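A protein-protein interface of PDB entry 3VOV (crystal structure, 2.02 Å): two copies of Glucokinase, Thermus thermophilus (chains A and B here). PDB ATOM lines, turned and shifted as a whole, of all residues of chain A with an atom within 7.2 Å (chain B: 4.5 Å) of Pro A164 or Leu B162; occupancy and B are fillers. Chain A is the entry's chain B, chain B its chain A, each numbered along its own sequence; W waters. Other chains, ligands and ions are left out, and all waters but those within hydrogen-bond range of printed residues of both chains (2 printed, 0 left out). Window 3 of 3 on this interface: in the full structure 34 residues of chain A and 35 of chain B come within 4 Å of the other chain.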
ATOM      1  N   THR A 161      -2.086  32.290   1.415  1.00  0.00           N
ATOM      2  CA  THR A 161      -0.679  32.241   1.119  1.00  0.00           C
ATOM      3  C   THR A 161      -0.493  31.550  -0.259  1.00  0.00           C
ATOM      4  O   THR A 161      -0.749  30.371  -0.370  1.00  0.00           O
ATOM      5  CB  THR A 161       0.044  31.449   2.206  1.00  0.00           C
ATOM      6  OG1 THR A 161      -0.184  32.077   3.470  1.00  0.00           O
ATOM      7  CG2 THR A 161       1.587  31.387   1.926  1.00  0.00           C
ATOM      8  N   LEU A 162       0.011  32.254  -1.255  1.00  0.00           N
ATOM      9  CA  LEU A 162       0.295  31.617  -2.527  1.00  0.00           C
ATOM     10  C   LEU A 162       1.779  31.428  -2.764  1.00  0.00           C
ATOM     11  O   LEU A 162       2.160  30.646  -3.626  1.00  0.00           O
ATOM     12  CB  LEU A 162      -0.207  32.484  -3.677  1.00  0.00           C
ATOM     13  CG  LEU A 162      -1.711  32.717  -3.727  1.00  0.00           C
ATOM     14  CD1 LEU A 162      -1.983  33.518  -4.970  1.00  0.00           C
ATOM     15  CD2 LEU A 162      -2.449  31.343  -3.744  1.00  0.00           C
ATOM     16  N   LEU A 163       2.612  32.221  -2.097  1.00  0.00           N
ATOM     17  CA  LEU A 163       4.053  32.060  -2.305  1.00  0.00           C
ATOM     18  C   LEU A 163       4.818  32.111  -0.979  1.00  0.00           C
ATOM     19  O   LEU A 163       5.264  33.177  -0.549  1.00  0.00           O
ATOM     20  CB  LEU A 163       4.591  33.102  -3.334  1.00  0.00           C
ATOM     21  CG  LEU A 163       6.086  32.977  -3.703  1.00  0.00           C
ATOM     22  CD1 LEU A 163       6.335  31.767  -4.652  1.00  0.00           C
ATOM     23  CD2 LEU A 163       6.614  34.258  -4.327  1.00  0.00           C
ATOM     24  N   PRO A 164       5.026  30.945  -0.352  1.00  0.00           N
ATOM     25  CA  PRO A 164       5.847  30.903   0.876  1.00  0.00           C
ATOM     26  C   PRO A 164       7.231  31.482   0.584  1.00  0.00           C
ATOM     27  O   PRO A 164       7.841  31.168  -0.430  1.00  0.00           O
ATOM     28  CB  PRO A 164       5.923  29.390   1.205  1.00  0.00           C
ATOM     29  CG  PRO A 164       4.683  28.798   0.541  1.00  0.00           C
ATOM     30  CD  PRO A 164       4.564  29.589  -0.758  1.00  0.00           C
ATOM     31  N   GLY A 165       7.700  32.378   1.435  1.00  0.00           N
ATOM     32  CA  GLY A 165       8.983  33.035   1.189  1.00  0.00           C
ATOM     33  C   GLY A 165       8.884  34.194   0.205  1.00  0.00           C
ATOM     34  O   GLY A 165       9.915  34.766  -0.199  1.00  0.00           O
ATOM     35  N   GLY A 166       7.653  34.544  -0.183  1.00  0.00           N
ATOM     36  CA  GLY A 166       7.381  35.732  -0.972  1.00  0.00           C
ATOM     37  C   GLY A 166       7.479  37.077  -0.198  1.00  0.00           C
ATOM     38  O   GLY A 166       7.963  37.141   0.931  1.00  0.00           O
ATOM     39  N   PRO A 167       7.030  38.159  -0.809  1.00  0.00           N
ATOM     40  CA  PRO A 167       7.207  39.493  -0.208  1.00  0.00           C
ATOM     41  C   PRO A 167       6.288  39.709   0.953  1.00  0.00           C
ATOM     42  O   PRO A 167       5.138  39.259   0.929  1.00  0.00           O
ATOM     43  CB  PRO A 167       6.825  40.467  -1.332  1.00  0.00           C
ATOM     44  CG  PRO A 167       6.637  39.611  -2.561  1.00  0.00           C
ATOM     45  CD  PRO A 167       6.336  38.218  -2.108  1.00  0.00           C
ATOM     46  N   GLU A 174       3.633  36.737   4.590  1.00  0.00           N
ATOM     47  CA  GLU A 174       4.406  37.034   3.370  1.00  0.00           C
ATOM     48  C   GLU A 174       3.840  36.158   2.259  1.00  0.00           C
ATOM     49  O   GLU A 174       3.323  35.096   2.534  1.00  0.00           O
ATOM     50  CB  GLU A 174       5.907  36.746   3.596  1.00  0.00           C
ATOM     51  CG  GLU A 174       6.400  35.344   3.118  1.00  0.00           C
ATOM     52  CD  GLU A 174       6.005  34.200   4.050  1.00  0.00           C
ATOM     53  OE1 GLU A 174       5.557  34.431   5.222  1.00  0.00           O
ATOM     54  OE2 GLU A 174       6.178  33.040   3.622  1.00  0.00           O
ATOM     55  N   GLY A 175       3.924  36.602   1.016  1.00  0.00           N
ATOM     56  CA  GLY A 175       3.456  35.770  -0.082  1.00  0.00           C
ATOM     57  C   GLY A 175       1.951  35.647  -0.216  1.00  0.00           C
ATOM     58  O   GLY A 175       1.481  34.737  -0.904  1.00  0.00           O
ATOM     59  N   CYS A 176       1.199  36.523   0.486  1.00  0.00           N
ATOM     60  CA  CYS A 176      -0.255  36.613   0.380  1.00  0.00           C
ATOM     61  C   CYS A 176      -0.593  37.050  -1.016  1.00  0.00           C
ATOM     62  O   CYS A 176       0.172  37.788  -1.642  1.00  0.00           O
ATOM     63  CB  CYS A 176      -0.785  37.663   1.385  1.00  0.00           C
ATOM     64  SG  CYS A 176      -0.670  37.090   3.042  1.00  0.00           S
ATOM     65  N   LEU A 180       1.265  40.055  -3.441  1.00  0.00           N
ATOM     66  CA  LEU A 180       1.820  39.681  -4.740  1.00  0.00           C
ATOM     67  C   LEU A 180       1.255  40.484  -5.878  1.00  0.00           C
ATOM     68  O   LEU A 180       1.943  40.682  -6.893  1.00  0.00           O
ATOM     69  CB  LEU A 180       1.519  38.200  -5.043  1.00  0.00           C
ATOM     70  CG  LEU A 180       2.287  37.201  -4.134  1.00  0.00           C
ATOM     71  CD1 LEU A 180       1.686  35.790  -4.358  1.00  0.00           C
ATOM     72  CD2 LEU A 180       3.858  37.210  -4.360  1.00  0.00           C
ATOM     73  N   ILE A 227      -4.180  32.015 -10.239  1.00  0.00           N
ATOM     74  CA  ILE A 227      -3.871  30.870  -9.407  1.00  0.00           C
ATOM     75  C   ILE A 227      -4.646  30.931  -8.094  1.00  0.00           C
ATOM     76  O   ILE A 227      -5.130  29.883  -7.597  1.00  0.00           O
ATOM     77  CB  ILE A 227      -2.333  30.776  -9.100  1.00  0.00           C
ATOM     78  CG1 ILE A 227      -1.561  30.461 -10.387  1.00  0.00           C
ATOM     79  CG2 ILE A 227      -2.049  29.675  -8.017  1.00  0.00           C
ATOM     80  CD1 ILE A 227       0.002  30.598 -10.203  1.00  0.00           C
ATOM     81  N   SER A 231      -7.436  28.200  -6.810  1.00  0.00           N
ATOM     82  CA  SER A 231      -7.186  27.516  -5.546  1.00  0.00           C
ATOM     83  C   SER A 231      -8.435  27.636  -4.632  1.00  0.00           C
ATOM     84  O   SER A 231      -8.917  26.654  -4.015  1.00  0.00           O
ATOM     85  CB  SER A 231      -5.948  28.163  -4.901  1.00  0.00           C
ATOM     86  OG  SER A 231      -5.239  27.279  -4.079  1.00  0.00           O
ATOM     87  N   LEU B 160      -5.654  22.759  -2.645  1.00  0.00           N
ATOM     88  CA  LEU B 160      -5.204  24.169  -2.675  1.00  0.00           C
ATOM     89  C   LEU B 160      -3.729  24.209  -3.063  1.00  0.00           C
ATOM     90  O   LEU B 160      -2.938  23.407  -2.589  1.00  0.00           O
ATOM     91  CB  LEU B 160      -5.442  24.864  -1.330  1.00  0.00           C
ATOM     92  CG  LEU B 160      -6.920  25.396  -1.424  1.00  0.00           C
ATOM     93  CD1 LEU B 160      -7.905  24.387  -0.786  1.00  0.00           C
ATOM     94  CD2 LEU B 160      -7.148  26.794  -0.845  1.00  0.00           C
ATOM     95  N   THR B 161      -3.375  25.153  -3.924  1.00  0.00           N
ATOM     96  CA  THR B 161      -2.018  25.308  -4.412  1.00  0.00           C
ATOM     97  C   THR B 161      -1.181  26.029  -3.351  1.00  0.00           C
ATOM     98  O   THR B 161      -1.459  27.176  -3.054  1.00  0.00           O
ATOM     99  CB  THR B 161      -2.022  26.171  -5.699  1.00  0.00           C
ATOM    100  OG1 THR B 161      -2.840  25.532  -6.685  1.00  0.00           O
ATOM    101  CG2 THR B 161      -0.580  26.386  -6.244  1.00  0.00           C
ATOM    102  N   LEU B 162      -0.174  25.360  -2.802  1.00  0.00           N
ATOM    103  CA  LEU B 162       0.740  25.969  -1.820  1.00  0.00           C
ATOM    104  C   LEU B 162       2.125  26.278  -2.421  1.00  0.00           C
ATOM    105  O   LEU B 162       2.848  27.118  -1.927  1.00  0.00           O
ATOM    106  CB  LEU B 162       0.930  25.038  -0.619  1.00  0.00           C
ATOM    107  CG  LEU B 162      -0.358  24.837   0.212  1.00  0.00           C
ATOM    108  CD1 LEU B 162      -0.024  24.063   1.512  1.00  0.00           C
ATOM    109  CD2 LEU B 162      -1.077  26.186   0.541  1.00  0.00           C
ATOM    110  N   LEU B 163       2.504  25.573  -3.476  1.00  0.00           N
ATOM    111  CA  LEU B 163       3.838  25.786  -4.030  1.00  0.00           C
ATOM    112  C   LEU B 163       3.735  25.774  -5.543  1.00  0.00           C
ATOM    113  O   LEU B 163       3.836  24.741  -6.166  1.00  0.00           O
ATOM    114  CB  LEU B 163       4.816  24.718  -3.472  1.00  0.00           C
ATOM    115  CG  LEU B 163       6.285  24.830  -3.963  1.00  0.00           C
ATOM    116  CD1 LEU B 163       6.891  26.125  -3.397  1.00  0.00           C
ATOM    117  CD2 LEU B 163       7.071  23.656  -3.492  1.00  0.00           C
ATOM    118  N   PRO B 164       3.514  26.944  -6.158  1.00  0.00           N
ATOM    119  CA  PRO B 164       3.511  26.957  -7.614  1.00  0.00           C
ATOM    120  C   PRO B 164       4.871  26.475  -8.121  1.00  0.00           C
ATOM    121  O   PRO B 164       5.901  26.864  -7.577  1.00  0.00           O
ATOM    122  CB  PRO B 164       3.295  28.437  -7.946  1.00  0.00           C
ATOM    123  CG  PRO B 164       2.526  28.981  -6.710  1.00  0.00           C
ATOM    124  CD  PRO B 164       3.251  28.283  -5.577  1.00  0.00           C
ATOM    125  N   GLY B 175       2.079  21.192  -6.827  1.00  0.00           N
ATOM    126  CA  GLY B 175       2.267  22.028  -5.626  1.00  0.00           C
ATOM    127  C   GLY B 175       1.003  22.065  -4.747  1.00  0.00           C
ATOM    128  O   GLY B 175       0.885  22.936  -3.886  1.00  0.00           O
ATOM    129  N   LEU B 177      -1.316  20.940  -1.724  1.00  0.00           N
ATOM    130  CA  LEU B 177      -1.088  20.377  -0.382  1.00  0.00           C
ATOM    131  C   LEU B 177      -0.940  18.838  -0.397  1.00  0.00           C
ATOM    132  O   LEU B 177      -0.007  18.293   0.198  1.00  0.00           O
ATOM    133  CB  LEU B 177      -2.261  20.767   0.539  1.00  0.00           C
ATOM    134  CG  LEU B 177      -2.208  20.276   1.980  1.00  0.00           C
ATOM    135  CD1 LEU B 177      -0.867  20.526   2.650  1.00  0.00           C
ATOM    136  CD2 LEU B 177      -3.344  21.007   2.798  1.00  0.00           C
ATOM    137  N   LEU B 180       2.328  17.745  -1.768  1.00  0.00           N
ATOM    138  CA  LEU B 180       3.469  18.061  -0.892  1.00  0.00           C
ATOM    139  C   LEU B 180       3.578  17.238   0.387  1.00  0.00           C
ATOM    140  O   LEU B 180       4.684  17.044   0.905  1.00  0.00           O
ATOM    141  CB  LEU B 180       3.431  19.545  -0.476  1.00  0.00           C
ATOM    142  CG  LEU B 180       3.507  20.598  -1.571  1.00  0.00           C
ATOM    143  CD1 LEU B 180       3.006  21.957  -1.051  1.00  0.00           C
ATOM    144  CD2 LEU B 180       4.965  20.647  -2.105  1.00  0.00           C
ATOM    145  N   TYR B 224       4.161  22.485   5.563  1.00  0.00           N
ATOM    146  CA  TYR B 224       3.176  22.693   4.484  1.00  0.00           C
ATOM    147  C   TYR B 224       1.737  22.480   4.983  1.00  0.00           C
ATOM    148  O   TYR B 224       0.822  23.218   4.623  1.00  0.00           O
ATOM    149  CB  TYR B 224       3.461  21.830   3.225  1.00  0.00           C
ATOM    150  CG  TYR B 224       4.509  22.473   2.318  1.00  0.00           C
ATOM    151  CD1 TYR B 224       4.390  23.824   1.895  1.00  0.00           C
ATOM    152  CD2 TYR B 224       5.626  21.753   1.900  1.00  0.00           C
ATOM    153  CE1 TYR B 224       5.371  24.403   1.074  1.00  0.00           C
ATOM    154  CE2 TYR B 224       6.607  22.326   1.050  1.00  0.00           C
ATOM    155  CZ  TYR B 224       6.468  23.635   0.651  1.00  0.00           C
ATOM    156  OH  TYR B 224       7.442  24.179  -0.147  1.00  0.00           O
ATOM    157  N   GLY B 228      -0.999  25.377   5.006  1.00  0.00           N
ATOM    158  CA  GLY B 228      -2.261  25.202   4.302  1.00  0.00           C
ATOM    159  C   GLY B 228      -3.448  25.427   5.214  1.00  0.00           C
ATOM    160  O   GLY B 228      -4.417  26.051   4.812  1.00  0.00           O
ATOM    161  N   TYR B 266       1.965  31.342  10.406  1.00  0.00           N
ATOM    162  CA  TYR B 266       1.125  31.820   9.282  1.00  0.00           C
ATOM    163  C   TYR B 266      -0.222  32.375   9.746  1.00  0.00           C
ATOM    164  O   TYR B 266      -1.139  32.677   8.926  1.00  0.00           O
ATOM    165  CB  TYR B 266       1.013  30.775   8.159  1.00  0.00           C
ATOM    166  CG  TYR B 266       2.260  30.817   7.320  1.00  0.00           C
ATOM    167  CD1 TYR B 266       2.303  31.524   6.124  1.00  0.00           C
ATOM    168  CD2 TYR B 266       3.430  30.220   7.769  1.00  0.00           C
ATOM    169  CE1 TYR B 266       3.492  31.603   5.378  1.00  0.00           C
ATOM    170  CE2 TYR B 266       4.606  30.296   7.035  1.00  0.00           C
ATOM    171  CZ  TYR B 266       4.631  30.984   5.852  1.00  0.00           C
ATOM    172  OH  TYR B 266       5.821  31.042   5.129  1.00  0.00           O
HETATM  173  O   HOH W   1      -3.691  28.614  -2.134  1.00  0.00           O
HETATM  174  O   HOH W   2       1.450  28.683   0.170  1.00  0.00           O
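The side-chain hydroxyl (OH) of Tyr B266 lies within hydrogen-bond range of the side-chain carboxylate (OE2) of Glu A174 (2.5 Å). N of Thr B161 lies within hydrogen-bond range of OG of Ser A231.
The backbone carbonyl oxygen (O) of Leu B160 is in hydrogen-bond range of the backbone NH (N) of Leu B177, at 3.1 Å. N of Gly A165 is in hydrogen-bond range of OE2 of Glu A174 (2.7 Å). The backbone NH (N) of Leu B162 sits at hydrogen-bond distance from the backbone carbonyl oxygen (O) of Gly B175. N of Leu A162 sits at hydrogen-bond distance from O of Gly A175 (2.9 Å).
Among the printed residues, merely in contact across the chains: Thr A161 with Tyr B266 (3.7 Å), Leu A162 with Leu B162 (3.98 Å), Leu A162 with Pro B164 (3.3 Å), Pro A164 with Leu B162 (3.2 Å) and Ser A231 with Leu B160 (3.4 Å).
Pro A164 touches just one residue of chain B: Leu B162 (3.2 Å). Of the printed residues of chain A, Leu B162 touches Leu A162 (3.98 Å) and Pro A164 (3.2 Å). Printed residues of chain B within 4 Å of Thr A161: Tyr B266 (3.7 Å). Printed residues of chain A within 4 Å of Pro B164: Leu A162. Printed residues of chain A within 4 Å of Leu B160: Ser A231 (3.4 Å). Ile A227 touches none of the printed residues of chain B.
Of the 13 printed residues of chain A, 5 touch a printed residue of chain B. Printed residues of chain A that touch a printed residue of chain B: Thr A161, Leu A162, Pro A164, Glu A174 and Ser A231. Hydrophobic or aromatic side chains of chain A that line the printed part of chain B: Pro A164. Of the 11 printed residues of chain B, 5 touch a printed residue of chain A. Printed residues of chain B that touch a printed residue of chain A: Leu B160, Thr B161, Leu B162, Pro B164 and Tyr B266. Hydrophobic or aromatic side chains of chain B that line the printed part of chain A: Leu B160, Pro B164 and Tyr B266.
Leu A162 touches its own counterpart, Leu B162. Leu A162 touches Pro B164, and with the chains exchanged Pro A164 touches Leu B162. 6 positions are printed for both chains.
Water W1 lies within hydrogen-bond range of the backbone carbonyl oxygen (O) of Thr B161 and the side-chain hydroxyl (OG) of Ser A231. Water W2 bridges the backbone carbonyl oxygen (O) of Thr A161 (2.8 Å) and the backbone carbonyl oxygen (O) of Leu B162 (3.0 Å).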
